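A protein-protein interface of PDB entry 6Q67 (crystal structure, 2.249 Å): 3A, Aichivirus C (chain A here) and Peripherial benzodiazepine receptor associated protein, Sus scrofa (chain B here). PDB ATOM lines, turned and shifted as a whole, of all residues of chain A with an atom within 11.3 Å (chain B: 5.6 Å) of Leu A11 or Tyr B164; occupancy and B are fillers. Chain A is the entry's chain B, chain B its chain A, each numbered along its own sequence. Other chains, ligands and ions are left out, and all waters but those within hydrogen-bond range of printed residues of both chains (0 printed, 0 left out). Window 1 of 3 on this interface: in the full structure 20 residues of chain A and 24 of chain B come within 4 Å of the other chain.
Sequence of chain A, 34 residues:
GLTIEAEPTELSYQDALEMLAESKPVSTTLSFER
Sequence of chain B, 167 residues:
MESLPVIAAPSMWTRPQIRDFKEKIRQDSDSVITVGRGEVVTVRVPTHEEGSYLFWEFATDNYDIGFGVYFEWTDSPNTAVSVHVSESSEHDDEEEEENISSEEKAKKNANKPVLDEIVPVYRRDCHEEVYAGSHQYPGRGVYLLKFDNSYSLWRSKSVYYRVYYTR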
ATOM      1  N   ALA A   6       5.411  29.915  -2.862  1.00  0.00           N
ATOM      2  CA  ALA A   6       6.839  29.642  -2.820  1.00  0.00           C
ATOM      3  C   ALA A   6       7.613  30.883  -3.203  1.00  0.00           C
ATOM      4  O   ALA A   6       7.240  31.602  -4.130  1.00  0.00           O
ATOM      5  CB  ALA A   6       7.191  28.496  -3.743  1.00  0.00           C
ATOM      6  N   GLU A   7       8.684  31.132  -2.467  1.00  0.00           N
ATOM      7  CA  GLU A   7       9.587  32.222  -2.776  1.00  0.00           C
ATOM      8  C   GLU A   7      10.767  31.647  -3.548  1.00  0.00           C
ATOM      9  O   GLU A   7      11.497  30.807  -3.026  1.00  0.00           O
ATOM     10  CB  GLU A   7      10.061  32.924  -1.501  1.00  0.00           C
ATOM     11  CG  GLU A   7      10.648  34.315  -1.740  1.00  0.00           C
ATOM     12  CD  GLU A   7       9.639  35.283  -2.342  1.00  0.00           C
ATOM     13  OE1 GLU A   7       8.424  35.085  -2.127  1.00  0.00           O
ATOM     14  OE2 GLU A   7      10.068  36.236  -3.034  1.00  0.00           O
ATOM     15  N   PRO A   8      10.959  32.087  -4.798  1.00  0.00           N
ATOM     16  CA  PRO A   8      12.045  31.507  -5.587  1.00  0.00           C
ATOM     17  C   PRO A   8      13.412  31.832  -4.996  1.00  0.00           C
ATOM     18  O   PRO A   8      13.572  32.852  -4.326  1.00  0.00           O
ATOM     19  CB  PRO A   8      11.872  32.165  -6.957  1.00  0.00           C
ATOM     20  CG  PRO A   8      11.247  33.474  -6.653  1.00  0.00           C
ATOM     21  CD  PRO A   8      10.322  33.221  -5.491  1.00  0.00           C
ATOM     22  N   THR A   9      14.383  30.968  -5.267  1.00  0.00           N
ATOM     23  CA  THR A   9      15.736  31.128  -4.759  1.00  0.00           C
ATOM     24  C   THR A   9      16.666  31.556  -5.889  1.00  0.00           C
ATOM     25  O   THR A   9      16.425  31.232  -7.050  1.00  0.00           O
ATOM     26  CB  THR A   9      16.252  29.826  -4.154  1.00  0.00           C
ATOM     27  OG1 THR A   9      16.425  28.861  -5.200  1.00  0.00           O
ATOM     28  CG2 THR A   9      15.267  29.290  -3.128  1.00  0.00           C
ATOM     29  N   GLU A  10      17.725  32.291  -5.568  1.00  0.00           N
ATOM     30  CA  GLU A  10      18.656  32.706  -6.610  1.00  0.00           C
ATOM     31  C   GLU A  10      19.339  31.488  -7.225  1.00  0.00           C
ATOM     32  O   GLU A  10      19.926  30.662  -6.520  1.00  0.00           O
ATOM     33  CB  GLU A  10      19.700  33.676  -6.065  1.00  0.00           C
ATOM     34  CG  GLU A  10      20.574  34.294  -7.149  1.00  0.00           C
ATOM     35  CD  GLU A  10      21.617  35.235  -6.586  1.00  0.00           C
ATOM     36  OE1 GLU A  10      21.243  36.197  -5.880  1.00  0.00           O
ATOM     37  OE2 GLU A  10      22.812  35.003  -6.852  1.00  0.00           O
ATOM     38  N   LEU A  11      19.246  31.382  -8.547  1.00  0.00           N
ATOM     39  CA  LEU A  11      19.901  30.316  -9.279  1.00  0.00           C
ATOM     40  C   LEU A  11      21.412  30.471  -9.132  1.00  0.00           C
ATOM     41  O   LEU A  11      21.923  31.581  -9.248  1.00  0.00           O
ATOM     42  CB  LEU A  11      19.508  30.354 -10.750  1.00  0.00           C
ATOM     43  CG  LEU A  11      19.905  29.111 -11.547  1.00  0.00           C
ATOM     44  CD1 LEU A  11      18.940  27.969 -11.269  1.00  0.00           C
ATOM     45  CD2 LEU A  11      19.963  29.415 -13.027  1.00  0.00           C
ATOM     46  N   SER A  12      22.108  29.361  -8.888  1.00  0.00           N
ATOM     47  CA  SER A  12      23.548  29.373  -8.615  1.00  0.00           C
ATOM     48  C   SER A  12      24.287  28.569  -9.656  1.00  0.00           C
ATOM     49  O   SER A  12      23.690  27.739 -10.332  1.00  0.00           O
ATOM     50  CB  SER A  12      23.851  28.787  -7.243  1.00  0.00           C
ATOM     51  OG  SER A  12      23.777  27.370  -7.301  1.00  0.00           O
ATOM     52  N   TYR A  13      25.588  28.807  -9.779  1.00  0.00           N
ATOM     53  CA  TYR A  13      26.387  28.102 -10.766  1.00  0.00           C
ATOM     54  C   TYR A  13      26.308  26.608 -10.513  1.00  0.00           C
ATOM     55  O   TYR A  13      26.258  25.829 -11.456  1.00  0.00           O
ATOM     56  CB  TYR A  13      27.846  28.568 -10.729  1.00  0.00           C
ATOM     57  CG  TYR A  13      28.744  27.935 -11.788  1.00  0.00           C
ATOM     58  CD1 TYR A  13      28.232  27.483 -12.996  1.00  0.00           C
ATOM     59  CD2 TYR A  13      30.113  27.796 -11.575  1.00  0.00           C
ATOM     60  CE1 TYR A  13      29.063  26.905 -13.966  1.00  0.00           C
ATOM     61  CE2 TYR A  13      30.951  27.224 -12.542  1.00  0.00           C
ATOM     62  CZ  TYR A  13      30.422  26.773 -13.729  1.00  0.00           C
ATOM     63  OH  TYR A  13      31.251  26.212 -14.693  1.00  0.00           O
ATOM     64  N   GLN A  14      26.316  26.213  -9.243  1.00  0.00           N
ATOM     65  CA  GLN A  14      26.156  24.808  -8.886  1.00  0.00           C
ATOM     66  C   GLN A  14      24.827  24.264  -9.426  1.00  0.00           C
ATOM     67  O   GLN A  14      24.820  23.284 -10.178  1.00  0.00           O
ATOM     68  CB  GLN A  14      26.214  24.614  -7.365  1.00  0.00           C
ATOM     69  CG  GLN A  14      25.871  23.187  -6.890  1.00  0.00           C
ATOM     70  CD  GLN A  14      27.090  22.365  -6.525  1.00  0.00           C
ATOM     71  OE1 GLN A  14      27.929  22.796  -5.738  1.00  0.00           O
ATOM     72  NE2 GLN A  14      27.184  21.164  -7.086  1.00  0.00           N
ATOM     73  N   ASP A  15      23.715  24.894  -9.041  1.00  0.00           N
ATOM     74  CA  ASP A  15      22.390  24.438  -9.470  1.00  0.00           C
ATOM     75  C   ASP A  15      22.407  24.223 -10.970  1.00  0.00           C
ATOM     76  O   ASP A  15      22.182  23.111 -11.449  1.00  0.00           O
ATOM     77  CB  ASP A  15      21.308  25.458  -9.124  1.00  0.00           C
ATOM     78  CG  ASP A  15      21.139  25.662  -7.632  1.00  0.00           C
ATOM     79  OD1 ASP A  15      21.101  24.664  -6.879  1.00  0.00           O
ATOM     80  OD2 ASP A  15      21.038  26.834  -7.214  1.00  0.00           O
ATOM     81  N   ALA A  16      22.771  25.286 -11.683  1.00  0.00           N
ATOM     82  CA  ALA A  16      22.784  25.308 -13.141  1.00  0.00           C
ATOM     83  C   ALA A  16      23.624  24.193 -13.751  1.00  0.00           C
ATOM     84  O   ALA A  16      23.360  23.778 -14.881  1.00  0.00           O
ATOM     85  CB  ALA A  16      23.293  26.657 -13.638  1.00  0.00           C
ATOM     86  N   LEU A  17      24.628  23.708 -13.025  1.00  0.00           N
ATOM     87  CA  LEU A  17      25.478  22.647 -13.558  1.00  0.00           C
ATOM     88  C   LEU A  17      24.669  21.389 -13.752  1.00  0.00           C
ATOM     89  O   LEU A  17      24.637  20.820 -14.846  1.00  0.00           O
ATOM     90  CB  LEU A  17      26.660  22.341 -12.636  1.00  0.00           C
ATOM     91  CG  LEU A  17      27.884  23.253 -12.715  1.00  0.00           C
ATOM     92  CD1 LEU A  17      28.900  22.853 -11.647  1.00  0.00           C
ATOM     93  CD2 LEU A  17      28.518  23.230 -14.107  1.00  0.00           C
ATOM     94  N   GLU A  18      24.031  20.963 -12.665  1.00  0.00           N
ATOM     95  CA  GLU A  18      23.233  19.748 -12.642  1.00  0.00           C
ATOM     96  C   GLU A  18      22.169  19.809 -13.723  1.00  0.00           C
ATOM     97  O   GLU A  18      22.067  18.905 -14.556  1.00  0.00           O
ATOM     98  CB  GLU A  18      22.589  19.563 -11.272  1.00  0.00           C
ATOM     99  CG  GLU A  18      23.588  19.508 -10.122  1.00  0.00           C
ATOM    100  CD  GLU A  18      22.926  19.633  -8.758  1.00  0.00           C
ATOM    101  OE1 GLU A  18      21.680  19.739  -8.702  1.00  0.00           O
ATOM    102  OE2 GLU A  18      23.654  19.627  -7.740  1.00  0.00           O
ATOM    103  N   MET A  19      21.415  20.910 -13.718  1.00  0.00           N
ATOM    104  CA  MET A  19      20.278  21.115 -14.623  1.00  0.00           C
ATOM    105  C   MET A  19      20.652  20.917 -16.073  1.00  0.00           C
ATOM    106  O   MET A  19      19.856  20.465 -16.898  1.00  0.00           O
ATOM    107  CB  MET A  19      19.717  22.532 -14.507  1.00  0.00           C
ATOM    108  CG  MET A  19      19.531  23.074 -13.111  1.00  0.00           C
ATOM    109  SD  MET A  19      18.224  24.321 -13.047  1.00  0.00           S
ATOM    110  CE  MET A  19      18.485  25.156 -14.617  1.00  0.00           C
ATOM    111  N   LEU A  20      21.865  21.332 -16.387  1.00  0.00           N
ATOM    112  CA  LEU A  20      22.353  21.267 -17.746  1.00  0.00           C
ATOM    113  C   LEU A  20      22.924  19.898 -18.112  1.00  0.00           C
ATOM    114  O   LEU A  20      23.013  19.538 -19.291  1.00  0.00           O
ATOM    115  CB  LEU A  20      23.408  22.335 -17.944  1.00  0.00           C
ATOM    116  CG  LEU A  20      24.159  22.183 -19.257  1.00  0.00           C
ATOM    117  CD1 LEU A  20      23.148  22.253 -20.450  1.00  0.00           C
ATOM    118  CD2 LEU A  20      25.248  23.204 -19.261  1.00  0.00           C
ATOM    119  N   PHE B  21      18.243  13.999  -8.320  1.00  0.00           N
ATOM    120  CA  PHE B  21      17.407  15.188  -8.152  1.00  0.00           C
ATOM    121  C   PHE B  21      16.481  15.016  -6.960  1.00  0.00           C
ATOM    122  O   PHE B  21      16.420  15.873  -6.084  1.00  0.00           O
ATOM    123  CB  PHE B  21      16.594  15.479  -9.417  1.00  0.00           C
ATOM    124  CG  PHE B  21      15.570  16.587  -9.250  1.00  0.00           C
ATOM    125  CD1 PHE B  21      15.968  17.917  -9.194  1.00  0.00           C
ATOM    126  CD2 PHE B  21      14.218  16.291  -9.153  1.00  0.00           C
ATOM    127  CE1 PHE B  21      15.045  18.929  -9.042  1.00  0.00           C
ATOM    128  CE2 PHE B  21      13.279  17.303  -9.005  1.00  0.00           C
ATOM    129  CZ  PHE B  21      13.693  18.622  -8.949  1.00  0.00           C
ATOM    130  N   TYR B  53      14.087  36.357 -14.664  1.00  0.00           N
ATOM    131  CA  TYR B  53      13.695  35.024 -15.135  1.00  0.00           C
ATOM    132  C   TYR B  53      13.180  34.138 -14.029  1.00  0.00           C
ATOM    133  O   TYR B  53      13.632  34.215 -12.886  1.00  0.00           O
ATOM    134  CB  TYR B  53      14.866  34.286 -15.785  1.00  0.00           C
ATOM    135  CG  TYR B  53      15.291  34.795 -17.131  1.00  0.00           C
ATOM    136  CD1 TYR B  53      16.221  35.827 -17.239  1.00  0.00           C
ATOM    137  CD2 TYR B  53      14.804  34.223 -18.291  1.00  0.00           C
ATOM    138  CE1 TYR B  53      16.636  36.287 -18.467  1.00  0.00           C
ATOM    139  CE2 TYR B  53      15.202  34.680 -19.529  1.00  0.00           C
ATOM    140  CZ  TYR B  53      16.127  35.713 -19.609  1.00  0.00           C
ATOM    141  OH  TYR B  53      16.546  36.182 -20.834  1.00  0.00           O
ATOM    142  N   LEU B  54      12.252  33.272 -14.413  1.00  0.00           N
ATOM    143  CA  LEU B  54      11.808  32.180 -13.576  1.00  0.00           C
ATOM    144  C   LEU B  54      12.426  30.915 -14.104  1.00  0.00           C
ATOM    145  O   LEU B  54      12.448  30.682 -15.313  1.00  0.00           O
ATOM    146  CB  LEU B  54      10.285  32.040 -13.583  1.00  0.00           C
ATOM    147  CG  LEU B  54       9.748  30.738 -12.983  1.00  0.00           C
ATOM    148  CD1 LEU B  54      10.038  30.653 -11.500  1.00  0.00           C
ATOM    149  CD2 LEU B  54       8.246  30.620 -13.214  1.00  0.00           C
ATOM    150  N   PHE B  55      12.892  30.090 -13.183  1.00  0.00           N
ATOM    151  CA  PHE B  55      13.380  28.764 -13.496  1.00  0.00           C
ATOM    152  C   PHE B  55      12.630  27.763 -12.653  1.00  0.00           C
ATOM    153  O   PHE B  55      12.445  28.003 -11.458  1.00  0.00           O
ATOM    154  CB  PHE B  55      14.866  28.666 -13.186  1.00  0.00           C
ATOM    155  CG  PHE B  55      15.751  28.834 -14.369  1.00  0.00           C
ATOM    156  CD1 PHE B  55      16.282  27.729 -14.993  1.00  0.00           C
ATOM    157  CD2 PHE B  55      16.085  30.094 -14.843  1.00  0.00           C
ATOM    158  CE1 PHE B  55      17.128  27.862 -16.078  1.00  0.00           C
ATOM    159  CE2 PHE B  55      16.939  30.236 -15.935  1.00  0.00           C
ATOM    160  CZ  PHE B  55      17.456  29.113 -16.548  1.00  0.00           C
ATOM    161  N   TRP B  56      12.218  26.645 -13.248  1.00  0.00           N
ATOM    162  CA  TRP B  56      11.589  25.578 -12.477  1.00  0.00           C
ATOM    163  C   TRP B  56      12.171  24.210 -12.819  1.00  0.00           C
ATOM    164  O   TRP B  56      12.533  23.945 -13.964  1.00  0.00           O
ATOM    165  CB  TRP B  56      10.064  25.558 -12.714  1.00  0.00           C
ATOM    166  CG  TRP B  56       9.681  25.188 -14.109  1.00  0.00           C
ATOM    167  CD1 TRP B  56       9.551  23.926 -14.623  1.00  0.00           C
ATOM    168  CD2 TRP B  56       9.372  26.091 -15.179  1.00  0.00           C
ATOM    169  NE1 TRP B  56       9.190  23.992 -15.957  1.00  0.00           N
ATOM    170  CE2 TRP B  56       9.074  25.313 -16.317  1.00  0.00           C
ATOM    171  CE3 TRP B  56       9.328  27.484 -15.288  1.00  0.00           C
ATOM    172  CZ2 TRP B  56       8.744  25.876 -17.539  1.00  0.00           C
ATOM    173  CZ3 TRP B  56       8.998  28.043 -16.510  1.00  0.00           C
ATOM    174  CH2 TRP B  56       8.711  27.241 -17.615  1.00  0.00           C
ATOM    175  N   GLU B  57      12.227  23.344 -11.811  1.00  0.00           N
ATOM    176  CA  GLU B  57      12.457  21.912 -12.009  1.00  0.00           C
ATOM    177  C   GLU B  57      11.449  21.095 -11.225  1.00  0.00           C
ATOM    178  O   GLU B  57      11.031  21.506 -10.143  1.00  0.00           O
ATOM    179  CB  GLU B  57      13.863  21.507 -11.554  1.00  0.00           C
ATOM    180  CG  GLU B  57      14.964  22.073 -12.363  1.00  0.00           C
ATOM    181  CD  GLU B  57      16.302  21.553 -11.896  1.00  0.00           C
ATOM    182  OE1 GLU B  57      16.668  21.823 -10.728  1.00  0.00           O
ATOM    183  OE2 GLU B  57      16.952  20.843 -12.692  1.00  0.00           O
ATOM    184  N   TYR B 137      10.639  37.002 -17.413  1.00  0.00           N
ATOM    185  CA  TYR B 137       9.564  37.774 -16.812  1.00  0.00           C
ATOM    186  C   TYR B 137       8.928  38.675 -17.865  1.00  0.00           C
ATOM    187  O   TYR B 137       9.625  39.479 -18.472  1.00  0.00           O
ATOM    188  CB  TYR B 137      10.085  38.636 -15.662  1.00  0.00           C
ATOM    189  CG  TYR B 137      10.524  37.902 -14.409  1.00  0.00           C
ATOM    190  CD1 TYR B 137      10.359  36.531 -14.276  1.00  0.00           C
ATOM    191  CD2 TYR B 137      11.091  38.598 -13.343  1.00  0.00           C
ATOM    192  CE1 TYR B 137      10.753  35.875 -13.111  1.00  0.00           C
ATOM    193  CE2 TYR B 137      11.487  37.947 -12.175  1.00  0.00           C
ATOM    194  CZ  TYR B 137      11.316  36.588 -12.068  1.00  0.00           C
ATOM    195  OH  TYR B 137      11.701  35.939 -10.911  1.00  0.00           O
ATOM    196  N   ARG B 162      11.489  22.530  -7.541  1.00  0.00           N
ATOM    197  CA  ARG B 162      12.281  23.700  -7.194  1.00  0.00           C
ATOM    198  C   ARG B 162      11.905  24.819  -8.139  1.00  0.00           C
ATOM    199  O   ARG B 162      11.733  24.589  -9.341  1.00  0.00           O
ATOM    200  CB  ARG B 162      13.790  23.425  -7.308  1.00  0.00           C
ATOM    201  CG  ARG B 162      14.443  22.796  -6.081  1.00  0.00           C
ATOM    202  CD  ARG B 162      15.377  23.759  -5.342  1.00  0.00           C
ATOM    203  NE  ARG B 162      15.740  23.276  -4.006  1.00  0.00           N
ATOM    204  CZ  ARG B 162      16.730  22.421  -3.747  1.00  0.00           C
ATOM    205  NH1 ARG B 162      17.474  21.926  -4.729  1.00  0.00           N
ATOM    206  NH2 ARG B 162      16.973  22.054  -2.494  1.00  0.00           N
ATOM    207  N   VAL B 163      11.787  26.025  -7.601  1.00  0.00           N
ATOM    208  CA  VAL B 163      11.667  27.217  -8.422  1.00  0.00           C
ATOM    209  C   VAL B 163      12.799  28.187  -8.098  1.00  0.00           C
ATOM    210  O   VAL B 163      13.190  28.333  -6.940  1.00  0.00           O
ATOM    211  CB  VAL B 163      10.337  27.915  -8.217  1.00  0.00           C
ATOM    212  CG1 VAL B 163       9.217  27.066  -8.789  1.00  0.00           C
ATOM    213  CG2 VAL B 163      10.117  28.189  -6.743  1.00  0.00           C
ATOM    214  N   TYR B 164      13.319  28.840  -9.131  1.00  0.00           N
ATOM    215  CA  TYR B 164      14.413  29.791  -8.969  1.00  0.00           C
ATOM    216  C   TYR B 164      14.134  31.096  -9.717  1.00  0.00           C
ATOM    217  O   TYR B 164      13.259  31.155 -10.588  1.00  0.00           O
ATOM    218  CB  TYR B 164      15.740  29.218  -9.500  1.00  0.00           C
ATOM    219  CG  TYR B 164      16.093  27.768  -9.171  1.00  0.00           C
ATOM    220  CD1 TYR B 164      16.961  27.463  -8.128  1.00  0.00           C
ATOM    221  CD2 TYR B 164      15.617  26.711  -9.948  1.00  0.00           C
ATOM    222  CE1 TYR B 164      17.322  26.148  -7.841  1.00  0.00           C
ATOM    223  CE2 TYR B 164      15.974  25.386  -9.665  1.00  0.00           C
ATOM    224  CZ  TYR B 164      16.830  25.116  -8.608  1.00  0.00           C
ATOM    225  OH  TYR B 164      17.197  23.817  -8.301  1.00  0.00           O
ATOM    226  N   TYR B 165      14.906  32.127  -9.379  1.00  0.00           N
ATOM    227  CA  TYR B 165      15.018  33.328 -10.202  1.00  0.00           C
ATOM    228  C   TYR B 165      16.490  33.564 -10.620  1.00  0.00           C
ATOM    229  O   TYR B 165      17.406  33.082  -9.960  1.00  0.00           O
ATOM    230  CB  TYR B 165      14.477  34.544  -9.451  1.00  0.00           C
ATOM    231  CG  TYR B 165      15.390  35.068  -8.351  1.00  0.00           C
ATOM    232  CD1 TYR B 165      16.310  36.083  -8.602  1.00  0.00           C
ATOM    233  CD2 TYR B 165      15.322  34.559  -7.059  1.00  0.00           C
ATOM    234  CE1 TYR B 165      17.138  36.570  -7.597  1.00  0.00           C
ATOM    235  CE2 TYR B 165      16.147  35.042  -6.048  1.00  0.00           C
ATOM    236  CZ  TYR B 165      17.051  36.047  -6.325  1.00  0.00           C
ATOM    237  OH  TYR B 165      17.870  36.527  -5.327  1.00  0.00           O
ATOM    238  N   THR B 166      16.705  34.286 -11.719  1.00  0.00           N
ATOM    239  CA  THR B 166      18.044  34.656 -12.155  1.00  0.00           C
ATOM    240  C   THR B 166      17.985  35.871 -13.069  1.00  0.00           C
ATOM    241  O   THR B 166      16.911  36.272 -13.504  1.00  0.00           O
ATOM    242  CB  THR B 166      18.755  33.509 -12.884  1.00  0.00           C
ATOM    243  OG1 THR B 166      20.069  33.928 -13.282  1.00  0.00           O
ATOM    244  CG2 THR B 166      17.987  33.100 -14.103  1.00  0.00           C
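The side-chain hydroxyl (OH) of Tyr B165 sits at hydrogen-bond distance from the side-chain carboxylate (OE1) of Glu A10 (3.4 Å). The side-chain sulfur of Met A19 lies close to the side-chain carboxylate of Glu B57. O of Tyr B165 is in hydrogen-bond range of N of Leu A11 (2.9 Å). The backbone NH (N) of Thr A9 is in hydrogen-bond range of the backbone carbonyl oxygen (O) of Val B163 (3.3 Å). The backbone NH of Tyr B165 lies within hydrogen-bond range of the backbone carbonyl oxygen of Thr A9, 2.9 Å away.
N of Glu B57 sits at hydrogen-bond distance from O of Arg B162 (2.8 Å). N of Tyr B164 is in hydrogen-bond range of O of Phe B55 (2.6 Å). The side-chain carboxylate of Asp A15 is in hydrogen-bond range of the side-chain hydroxyl of Ser A12. OH of Tyr B164 is in hydrogen-bond range of OE1 of Glu B57. The backbone NH (N) of Tyr B53 sits at hydrogen-bond distance from the backbone carbonyl oxygen (O) of Thr B166, 3.1 Å away.
Val B163 touches Pro A8 (O to CA, 3.6 Å). Pro A8 touches Tyr B164. Pro A8 touches Tyr B165 (O to CD2, 3.7 Å). Thr A9 touches Tyr B164. Leu A11 touches Tyr B164. Leu A11 touches Thr B166. CE1 of Tyr B164 touches OD2 of Asp A15, 3.8 Å away. Met A19 touches Phe B55 (CE to CE1, 3.4 Å).
Of chain A, only Pro A8 (3.7 Å), Thr A9 (3.1 Å), Leu A11 (3.5 Å) and Asp A15 (3.8 Å) come within 4 Å of Tyr B164. Leu B54 touches none of the printed residues of chain A. Phe B55 touches just one residue of chain A: Met A19. Of chain A, only Met A19 comes within 4 Å of Glu B57. No residue of chain A comes within 4 Å of Arg B162. Of chain A, only Pro A8, Thr A9, Glu A10 and Leu A11 come within 4 Å of Tyr B165. Thr B166 touches just one residue of chain A: Leu A11 (3.9 Å). Of the printed residues of chain B, Thr A9 touches Val B163 (3.3 Å), Tyr B164 (3.1 Å) and Tyr B165 (2.9 Å). Of the printed residues of chain B, Glu A10 touches Tyr B165 (3.2 Å). Printed residues of chain B within 4 Å of Met A19: Phe B55 (3.4 Å) and Glu B57 (3.4 Å). Tyr B137 touches none of the printed residues of chain A. Phe B21 touches none of the printed residues of chain A.
Printed residues of chain A that touch a printed residue of chain B: Pro A8, Thr A9, Glu A10, Leu A11, Asp A15 and Met A19. Along chain A the printed residues that touch a printed residue of chain B span positions 8 to 19. Of the 12 printed residues of chain B, 6 touch a printed residue of chain A. Printed residues of chain B that touch a printed residue of chain A: Phe B55, Glu B57, Val B163, Tyr B164, Tyr B165 and Thr B166. Hydrophobic or aromatic side chains of chain B within 4 Å of the printed part of chain A: Phe B55, Tyr B164 and Tyr B165. Among the printed residues, 13 pairs touch across the chains. Among the printed residues, no Asp or Glu carboxylate lies within 4 Å of a Lys or Arg side-chain nitrogen of the other chain.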
